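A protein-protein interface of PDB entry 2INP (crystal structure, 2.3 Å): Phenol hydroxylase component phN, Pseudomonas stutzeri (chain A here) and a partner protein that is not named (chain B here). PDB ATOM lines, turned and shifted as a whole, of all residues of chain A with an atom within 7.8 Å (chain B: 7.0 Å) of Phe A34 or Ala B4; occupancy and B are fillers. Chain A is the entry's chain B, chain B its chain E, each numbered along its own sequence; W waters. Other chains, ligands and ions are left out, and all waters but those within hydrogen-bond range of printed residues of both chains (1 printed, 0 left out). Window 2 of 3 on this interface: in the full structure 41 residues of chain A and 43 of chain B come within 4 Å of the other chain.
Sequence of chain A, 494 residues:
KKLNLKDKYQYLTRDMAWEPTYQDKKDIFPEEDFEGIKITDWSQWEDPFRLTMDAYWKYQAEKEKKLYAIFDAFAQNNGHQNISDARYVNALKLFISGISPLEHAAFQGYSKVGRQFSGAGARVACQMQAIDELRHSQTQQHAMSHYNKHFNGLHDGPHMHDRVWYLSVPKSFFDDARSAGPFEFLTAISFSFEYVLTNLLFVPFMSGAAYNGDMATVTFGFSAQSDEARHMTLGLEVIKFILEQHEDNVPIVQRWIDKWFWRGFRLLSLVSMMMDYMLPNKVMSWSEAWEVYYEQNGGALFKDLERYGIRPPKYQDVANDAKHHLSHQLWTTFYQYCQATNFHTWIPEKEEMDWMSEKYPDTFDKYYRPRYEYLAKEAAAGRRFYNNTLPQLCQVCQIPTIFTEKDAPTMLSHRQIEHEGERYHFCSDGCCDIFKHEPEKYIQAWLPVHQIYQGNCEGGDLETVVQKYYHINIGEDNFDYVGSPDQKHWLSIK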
ATOM      1  N   LYS A  26       1.556 -31.111  -8.794  1.00  0.00           N
ATOM      2  CA  LYS A  26       1.301 -30.068  -7.793  1.00  0.00           C
ATOM      3  C   LYS A  26       1.457 -28.678  -8.346  1.00  0.00           C
ATOM      4  O   LYS A  26       1.066 -27.734  -7.711  1.00  0.00           O
ATOM      5  CB  LYS A  26       2.083 -30.297  -6.473  1.00  0.00           C
ATOM      6  CG  LYS A  26       1.678 -31.613  -5.735  1.00  0.00           C
ATOM      7  CD  LYS A  26       0.796 -31.368  -4.519  1.00  0.00           C
ATOM      8  CE  LYS A  26      -0.094 -32.577  -4.083  1.00  0.00           C
ATOM      9  NZ  LYS A  26      -1.427 -32.122  -3.384  1.00  0.00           N
ATOM     10  N   PRO A  30      -2.102 -26.694  -7.573  1.00  0.00           N
ATOM     11  CA  PRO A  30      -1.400 -26.065  -6.411  1.00  0.00           C
ATOM     12  C   PRO A  30      -2.293 -25.627  -5.217  1.00  0.00           C
ATOM     13  O   PRO A  30      -1.779 -25.072  -4.202  1.00  0.00           O
ATOM     14  CB  PRO A  30      -0.725 -24.836  -7.051  1.00  0.00           C
ATOM     15  CG  PRO A  30      -1.841 -24.357  -8.145  1.00  0.00           C
ATOM     16  CD  PRO A  30      -2.385 -25.732  -8.675  1.00  0.00           C
ATOM     17  N   GLU A  31      -3.597 -25.855  -5.299  1.00  0.00           N
ATOM     18  CA  GLU A  31      -4.526 -25.340  -4.249  1.00  0.00           C
ATOM     19  C   GLU A  31      -5.080 -26.363  -3.249  1.00  0.00           C
ATOM     20  O   GLU A  31      -5.785 -26.021  -2.266  1.00  0.00           O
ATOM     21  CB  GLU A  31      -5.695 -24.580  -4.889  1.00  0.00           C
ATOM     22  CG  GLU A  31      -5.275 -23.274  -5.474  1.00  0.00           C
ATOM     23  CD  GLU A  31      -6.478 -22.442  -6.008  1.00  0.00           C
ATOM     24  OE1 GLU A  31      -7.644 -22.631  -5.524  1.00  0.00           O
ATOM     25  OE2 GLU A  31      -6.231 -21.608  -6.921  1.00  0.00           O
ATOM     26  N   GLU A  32      -4.760 -27.620  -3.512  1.00  0.00           N
ATOM     27  CA  GLU A  32      -5.212 -28.750  -2.724  1.00  0.00           C
ATOM     28  C   GLU A  32      -4.559 -29.107  -1.374  1.00  0.00           C
ATOM     29  O   GLU A  32      -5.128 -29.931  -0.648  1.00  0.00           O
ATOM     30  CB  GLU A  32      -5.151 -29.938  -3.605  1.00  0.00           C
ATOM     31  CG  GLU A  32      -6.251 -29.910  -4.663  1.00  0.00           C
ATOM     32  CD  GLU A  32      -6.362 -31.209  -5.332  1.00  0.00           C
ATOM     33  OE1 GLU A  32      -7.473 -31.595  -5.665  1.00  0.00           O
ATOM     34  OE2 GLU A  32      -5.305 -31.845  -5.550  1.00  0.00           O
ATOM     35  N   ASP A  33      -3.457 -28.461  -0.982  1.00  0.00           N
ATOM     36  CA  ASP A  33      -2.696 -28.873   0.203  1.00  0.00           C
ATOM     37  C   ASP A  33      -2.782 -27.901   1.361  1.00  0.00           C
ATOM     38  O   ASP A  33      -2.712 -28.299   2.543  1.00  0.00           O
ATOM     39  CB  ASP A  33      -1.227 -29.017  -0.125  1.00  0.00           C
ATOM     40  CG  ASP A  33      -0.954 -30.127  -1.110  1.00  0.00           C
ATOM     41  OD1 ASP A  33      -0.231 -29.838  -2.090  1.00  0.00           O
ATOM     42  OD2 ASP A  33      -1.469 -31.277  -0.938  1.00  0.00           O
ATOM     43  N   PHE A  34      -2.956 -26.627   1.048  1.00  0.00           N
ATOM     44  CA  PHE A  34      -2.711 -25.590   2.025  1.00  0.00           C
ATOM     45  C   PHE A  34      -3.765 -25.427   3.125  1.00  0.00           C
ATOM     46  O   PHE A  34      -3.522 -24.752   4.147  1.00  0.00           O
ATOM     47  CB  PHE A  34      -2.455 -24.264   1.276  1.00  0.00           C
ATOM     48  CG  PHE A  34      -3.688 -23.583   0.762  1.00  0.00           C
ATOM     49  CD1 PHE A  34      -4.369 -22.698   1.556  1.00  0.00           C
ATOM     50  CD2 PHE A  34      -4.141 -23.808  -0.538  1.00  0.00           C
ATOM     51  CE1 PHE A  34      -5.497 -22.054   1.118  1.00  0.00           C
ATOM     52  CE2 PHE A  34      -5.311 -23.105  -1.014  1.00  0.00           C
ATOM     53  CZ  PHE A  34      -5.943 -22.249  -0.171  1.00  0.00           C
ATOM     54  N   GLU A  35      -4.948 -25.987   2.870  1.00  0.00           N
ATOM     55  CA  GLU A  35      -6.084 -25.980   3.815  1.00  0.00           C
ATOM     56  C   GLU A  35      -5.995 -27.024   4.917  1.00  0.00           C
ATOM     57  O   GLU A  35      -6.723 -26.925   5.890  1.00  0.00           O
ATOM     58  CB  GLU A  35      -7.384 -26.228   3.076  1.00  0.00           C
ATOM     59  CG  GLU A  35      -7.933 -24.965   2.460  1.00  0.00           C
ATOM     60  CD  GLU A  35      -9.079 -25.267   1.522  1.00  0.00           C
ATOM     61  OE1 GLU A  35      -8.843 -26.072   0.566  1.00  0.00           O
ATOM     62  OE2 GLU A  35     -10.201 -24.723   1.792  1.00  0.00           O
ATOM     63  N   GLY A  36      -5.086 -27.998   4.759  1.00  0.00           N
ATOM     64  CA  GLY A  36      -4.845 -29.035   5.793  1.00  0.00           C
ATOM     65  C   GLY A  36      -5.502 -30.360   5.389  1.00  0.00           C
ATOM     66  O   GLY A  36      -5.244 -31.401   6.029  1.00  0.00           O
ATOM     67  N   ILE A  37      -6.331 -30.316   4.327  1.00  0.00           N
ATOM     68  CA  ILE A  37      -7.132 -31.466   3.886  1.00  0.00           C
ATOM     69  C   ILE A  37      -6.289 -32.459   3.133  1.00  0.00           C
ATOM     70  O   ILE A  37      -5.429 -32.085   2.319  1.00  0.00           O
ATOM     71  CB  ILE A  37      -8.365 -31.036   3.000  1.00  0.00           C
ATOM     72  CG1 ILE A  37      -9.322 -30.154   3.811  1.00  0.00           C
ATOM     73  CG2 ILE A  37      -9.087 -32.233   2.375  1.00  0.00           C
ATOM     74  CD1 ILE A  37     -10.068 -30.830   5.006  1.00  0.00           C
ATOM     75  N   SER A 179     -12.725 -16.309  -1.346  1.00  0.00           N
ATOM     76  CA  SER A 179     -11.325 -16.056  -0.920  1.00  0.00           C
ATOM     77  C   SER A 179     -10.738 -17.278  -0.201  1.00  0.00           C
ATOM     78  O   SER A 179      -9.529 -17.433  -0.141  1.00  0.00           O
ATOM     79  CB  SER A 179     -11.201 -14.821  -0.083  1.00  0.00           C
ATOM     80  OG  SER A 179     -11.998 -14.929   1.060  1.00  0.00           O
ATOM     81  N   ALA A 180     -11.616 -18.165   0.270  1.00  0.00           N
ATOM     82  CA  ALA A 180     -11.199 -19.405   0.940  1.00  0.00           C
ATOM     83  C   ALA A 180     -10.686 -20.352  -0.086  1.00  0.00           C
ATOM     84  O   ALA A 180     -10.888 -20.165  -1.320  1.00  0.00           O
ATOM     85  CB  ALA A 180     -12.354 -20.039   1.705  1.00  0.00           C
ATOM     86  N   GLY A 181     -10.028 -21.393   0.391  1.00  0.00           N
ATOM     87  CA  GLY A 181      -9.597 -22.398  -0.494  1.00  0.00           C
ATOM     88  C   GLY A 181     -10.722 -23.283  -0.941  1.00  0.00           C
ATOM     89  O   GLY A 181     -11.909 -23.154  -0.519  1.00  0.00           O
ATOM     90  N   PRO A 182     -10.374 -24.226  -1.813  1.00  0.00           N
ATOM     91  CA  PRO A 182     -11.360 -24.974  -2.584  1.00  0.00           C
ATOM     92  C   PRO A 182     -12.185 -26.032  -1.791  1.00  0.00           C
ATOM     93  O   PRO A 182     -13.398 -26.184  -2.062  1.00  0.00           O
ATOM     94  CB  PRO A 182     -10.525 -25.576  -3.726  1.00  0.00           C
ATOM     95  CG  PRO A 182      -9.104 -25.687  -3.174  1.00  0.00           C
ATOM     96  CD  PRO A 182      -8.983 -24.571  -2.152  1.00  0.00           C
ATOM     97  N   PHE A 183     -11.592 -26.699  -0.786  1.00  0.00           N
ATOM     98  CA  PHE A 183     -12.397 -27.651   0.050  1.00  0.00           C
ATOM     99  C   PHE A 183     -13.312 -26.896   0.981  1.00  0.00           C
ATOM    100  O   PHE A 183     -14.427 -27.368   1.303  1.00  0.00           O
ATOM    101  CB  PHE A 183     -11.502 -28.592   0.872  1.00  0.00           C
ATOM    102  CG  PHE A 183     -10.696 -29.548   0.027  1.00  0.00           C
ATOM    103  CD1 PHE A 183      -9.314 -29.355  -0.148  1.00  0.00           C
ATOM    104  CD2 PHE A 183     -11.329 -30.601  -0.634  1.00  0.00           C
ATOM    105  CE1 PHE A 183      -8.558 -30.222  -0.956  1.00  0.00           C
ATOM    106  CE2 PHE A 183     -10.598 -31.446  -1.448  1.00  0.00           C
ATOM    107  CZ  PHE A 183      -9.163 -31.247  -1.607  1.00  0.00           C
ATOM    108  N   GLU A 184     -12.853 -25.740   1.462  1.00  0.00           N
ATOM    109  CA  GLU A 184     -13.739 -24.883   2.261  1.00  0.00           C
ATOM    110  C   GLU A 184     -14.857 -24.290   1.391  1.00  0.00           C
ATOM    111  O   GLU A 184     -15.983 -24.171   1.818  1.00  0.00           O
ATOM    112  CB  GLU A 184     -12.986 -23.740   2.956  1.00  0.00           C
ATOM    113  CG  GLU A 184     -13.937 -22.998   3.889  1.00  0.00           C
ATOM    114  CD  GLU A 184     -13.288 -21.882   4.671  1.00  0.00           C
ATOM    115  OE1 GLU A 184     -13.994 -21.329   5.502  1.00  0.00           O
ATOM    116  OE2 GLU A 184     -12.079 -21.576   4.476  1.00  0.00           O
ATOM    117  N   TRP A 256     -15.433 -25.947   9.697  1.00  0.00           N
ATOM    118  CA  TRP A 256     -16.070 -25.361   8.524  1.00  0.00           C
ATOM    119  C   TRP A 256     -17.557 -25.407   8.667  1.00  0.00           C
ATOM    120  O   TRP A 256     -18.235 -24.423   8.369  1.00  0.00           O
ATOM    121  CB  TRP A 256     -15.632 -26.015   7.213  1.00  0.00           C
ATOM    122  CG  TRP A 256     -14.300 -25.646   6.846  1.00  0.00           C
ATOM    123  CD1 TRP A 256     -13.536 -24.556   7.325  1.00  0.00           C
ATOM    124  CD2 TRP A 256     -13.458 -26.376   5.956  1.00  0.00           C
ATOM    125  NE1 TRP A 256     -12.261 -24.594   6.724  1.00  0.00           N
ATOM    126  CE2 TRP A 256     -12.204 -25.693   5.895  1.00  0.00           C
ATOM    127  CE3 TRP A 256     -13.644 -27.543   5.187  1.00  0.00           C
ATOM    128  CZ2 TRP A 256     -11.174 -26.138   5.089  1.00  0.00           C
ATOM    129  CZ3 TRP A 256     -12.622 -27.971   4.381  1.00  0.00           C
ATOM    130  CH2 TRP A 256     -11.399 -27.297   4.360  1.00  0.00           C
ATOM    131  N   GLU A 438      -9.936 -16.617  12.493  1.00  0.00           N
ATOM    132  CA  GLU A 438      -9.233 -16.019  11.295  1.00  0.00           C
ATOM    133  C   GLU A 438      -9.261 -14.467  11.362  1.00  0.00           C
ATOM    134  O   GLU A 438      -9.840 -13.782  10.498  1.00  0.00           O
ATOM    135  CB  GLU A 438      -9.760 -16.510   9.947  1.00  0.00           C
ATOM    136  CG  GLU A 438      -9.935 -17.968   9.754  1.00  0.00           C
ATOM    137  CD  GLU A 438     -10.746 -18.338   8.476  1.00  0.00           C
ATOM    138  OE1 GLU A 438     -10.116 -18.660   7.426  1.00  0.00           O
ATOM    139  OE2 GLU A 438     -12.005 -18.425   8.539  1.00  0.00           O
ATOM    140  N   SER B   1      -5.805 -19.304  13.167  1.00  0.00           N
ATOM    141  CA  SER B   1      -5.331 -18.432  12.067  1.00  0.00           C
ATOM    142  C   SER B   1      -5.621 -18.980  10.641  1.00  0.00           C
ATOM    143  O   SER B   1      -6.025 -20.139  10.450  1.00  0.00           O
ATOM    144  CB  SER B   1      -3.844 -18.117  12.267  1.00  0.00           C
ATOM    145  OG  SER B   1      -3.115 -19.300  12.126  1.00  0.00           O
ATOM    146  N   VAL B   2      -5.421 -18.103   9.656  1.00  0.00           N
ATOM    147  CA  VAL B   2      -5.772 -18.328   8.254  1.00  0.00           C
ATOM    148  C   VAL B   2      -4.832 -19.339   7.627  1.00  0.00           C
ATOM    149  O   VAL B   2      -3.605 -19.226   7.780  1.00  0.00           O
ATOM    150  CB  VAL B   2      -5.732 -16.957   7.441  1.00  0.00           C
ATOM    151  CG1 VAL B   2      -6.180 -17.146   6.039  1.00  0.00           C
ATOM    152  CG2 VAL B   2      -6.682 -15.949   8.057  1.00  0.00           C
ATOM    153  N   ASN B   3      -5.365 -20.333   6.936  1.00  0.00           N
ATOM    154  CA  ASN B   3      -4.563 -21.039   5.960  1.00  0.00           C
ATOM    155  C   ASN B   3      -4.586 -20.249   4.634  1.00  0.00           C
ATOM    156  O   ASN B   3      -5.681 -19.725   4.185  1.00  0.00           O
ATOM    157  CB  ASN B   3      -5.064 -22.459   5.766  1.00  0.00           C
ATOM    158  CG  ASN B   3      -5.058 -23.263   7.082  1.00  0.00           C
ATOM    159  OD1 ASN B   3      -4.320 -22.941   8.002  1.00  0.00           O
ATOM    160  ND2 ASN B   3      -5.918 -24.283   7.174  1.00  0.00           N
ATOM    161  N   ALA B   4      -3.393 -20.095   4.061  1.00  0.00           N
ATOM    162  CA  ALA B   4      -3.184 -19.338   2.856  1.00  0.00           C
ATOM    163  C   ALA B   4      -1.964 -19.955   2.285  1.00  0.00           C
ATOM    164  O   ALA B   4      -1.259 -20.688   2.981  1.00  0.00           O
ATOM    165  CB  ALA B   4      -2.911 -17.866   3.174  1.00  0.00           C
ATOM    166  N   LEU B   5      -1.688 -19.590   1.043  1.00  0.00           N
ATOM    167  CA  LEU B   5      -0.585 -20.057   0.248  1.00  0.00           C
ATOM    168  C   LEU B   5       0.595 -19.073   0.301  1.00  0.00           C
ATOM    169  O   LEU B   5       1.573 -19.200  -0.439  1.00  0.00           O
ATOM    170  CB  LEU B   5      -1.125 -20.118  -1.169  1.00  0.00           C
ATOM    171  CG  LEU B   5      -0.978 -21.254  -2.161  1.00  0.00           C
ATOM    172  CD1 LEU B   5      -0.909 -22.643  -1.477  1.00  0.00           C
ATOM    173  CD2 LEU B   5      -2.119 -21.099  -3.159  1.00  0.00           C
ATOM    174  N   TYR B   6       0.493 -18.060   1.156  1.00  0.00           N
ATOM    175  CA  TYR B   6       1.533 -17.057   1.322  1.00  0.00           C
ATOM    176  C   TYR B   6       1.277 -16.482   2.700  1.00  0.00           C
ATOM    177  O   TYR B   6       0.322 -16.912   3.416  1.00  0.00           O
ATOM    178  CB  TYR B   6       1.439 -15.994   0.250  1.00  0.00           C
ATOM    179  CG  TYR B   6       0.082 -15.281   0.192  1.00  0.00           C
ATOM    180  CD1 TYR B   6      -1.018 -15.854  -0.427  1.00  0.00           C
ATOM    181  CD2 TYR B   6      -0.090 -14.043   0.806  1.00  0.00           C
ATOM    182  CE1 TYR B   6      -2.289 -15.161  -0.475  1.00  0.00           C
ATOM    183  CE2 TYR B   6      -1.325 -13.361   0.790  1.00  0.00           C
ATOM    184  CZ  TYR B   6      -2.426 -13.903   0.112  1.00  0.00           C
ATOM    185  OH  TYR B   6      -3.604 -13.156   0.103  1.00  0.00           O
ATOM    186  N   ASP B   7       2.113 -15.528   3.108  1.00  0.00           N
ATOM    187  CA  ASP B   7       1.974 -15.001   4.446  1.00  0.00           C
ATOM    188  C   ASP B   7       0.826 -14.010   4.468  1.00  0.00           C
ATOM    189  O   ASP B   7       0.900 -12.917   3.906  1.00  0.00           O
ATOM    190  CB  ASP B   7       3.285 -14.410   4.981  1.00  0.00           C
ATOM    191  CG  ASP B   7       3.218 -14.214   6.487  1.00  0.00           C
ATOM    192  OD1 ASP B   7       3.008 -15.223   7.227  1.00  0.00           O
ATOM    193  OD2 ASP B   7       3.267 -13.054   6.939  1.00  0.00           O
ATOM    194  N   TYR B   8      -0.270 -14.413   5.078  1.00  0.00           N
ATOM    195  CA  TYR B   8      -1.532 -13.704   4.897  1.00  0.00           C
ATOM    196  C   TYR B   8      -1.640 -12.635   5.942  1.00  0.00           C
ATOM    197  O   TYR B   8      -2.056 -12.909   7.065  1.00  0.00           O
ATOM    198  CB  TYR B   8      -2.689 -14.720   5.055  1.00  0.00           C
ATOM    199  CG  TYR B   8      -4.027 -14.278   4.538  1.00  0.00           C
ATOM    200  CD1 TYR B   8      -4.354 -14.366   3.150  1.00  0.00           C
ATOM    201  CD2 TYR B   8      -5.001 -13.825   5.416  1.00  0.00           C
ATOM    202  CE1 TYR B   8      -5.577 -13.956   2.678  1.00  0.00           C
ATOM    203  CE2 TYR B   8      -6.239 -13.403   4.949  1.00  0.00           C
ATOM    204  CZ  TYR B   8      -6.521 -13.492   3.565  1.00  0.00           C
ATOM    205  OH  TYR B   8      -7.757 -13.081   3.118  1.00  0.00           O
HETATM  206  O   HOH W   1      -8.101 -20.385   7.007  1.00  0.00           O
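OE1 of Glu A35 is in hydrogen-bond range of N of Phe A183. The backbone NH (N) of Glu A184 lies within hydrogen-bond range of the side-chain carboxylate (OE2) of Glu A35, at 2.9 Å.
Printed residues of chain B within 4 Å of Phe A34: Asn B3, Ala B4 and Leu B5. Of chain A, only Phe A34 (3.7 Å) comes within 4 Å of Ala B4. Printed residues of chain B within 4 Å of Pro A30: Leu B5. Of the printed residues of chain B, Glu A438 touches Val B2. The nearest residue of chain B that does not touch Phe A34 is Val B2 (6.6 Å). The nearest residue of chain A that does not touch Ala B4 is Glu A35 (6.2 Å).
Of the 8 printed residues of chain B, 4 touch a printed residue of chain A. Printed residues of chain B that touch a printed residue of chain A: Val B2, Asn B3, Ala B4 and Leu B5. Hydrophobic or aromatic side chains of chain B within 4 Å of the printed part of chain A: Val B2 and Leu B5. Of the 17 printed residues of chain A, 4 touch a printed residue of chain B. Among the printed residues, 6 pairs touch across the chains.
Pro A30 touches Leu B5 (O to CD1, 3.8 Å). O of Phe A34 touches CB of Asn B3, at 3.2 Å. Phe A34 touches Ala B4 (CD1 to C, 3.7 Å). Leu B5 touches Phe A34. Glu A438 touches Val B2.
Water W1 lies within hydrogen-bond range of OE1 of Glu A438 (2.7 Å) and N of Asn B3 (2.7 Å).
O of Glu A35 sits at hydrogen-bond distance from ND2 of Asn B3 (3.0 Å).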
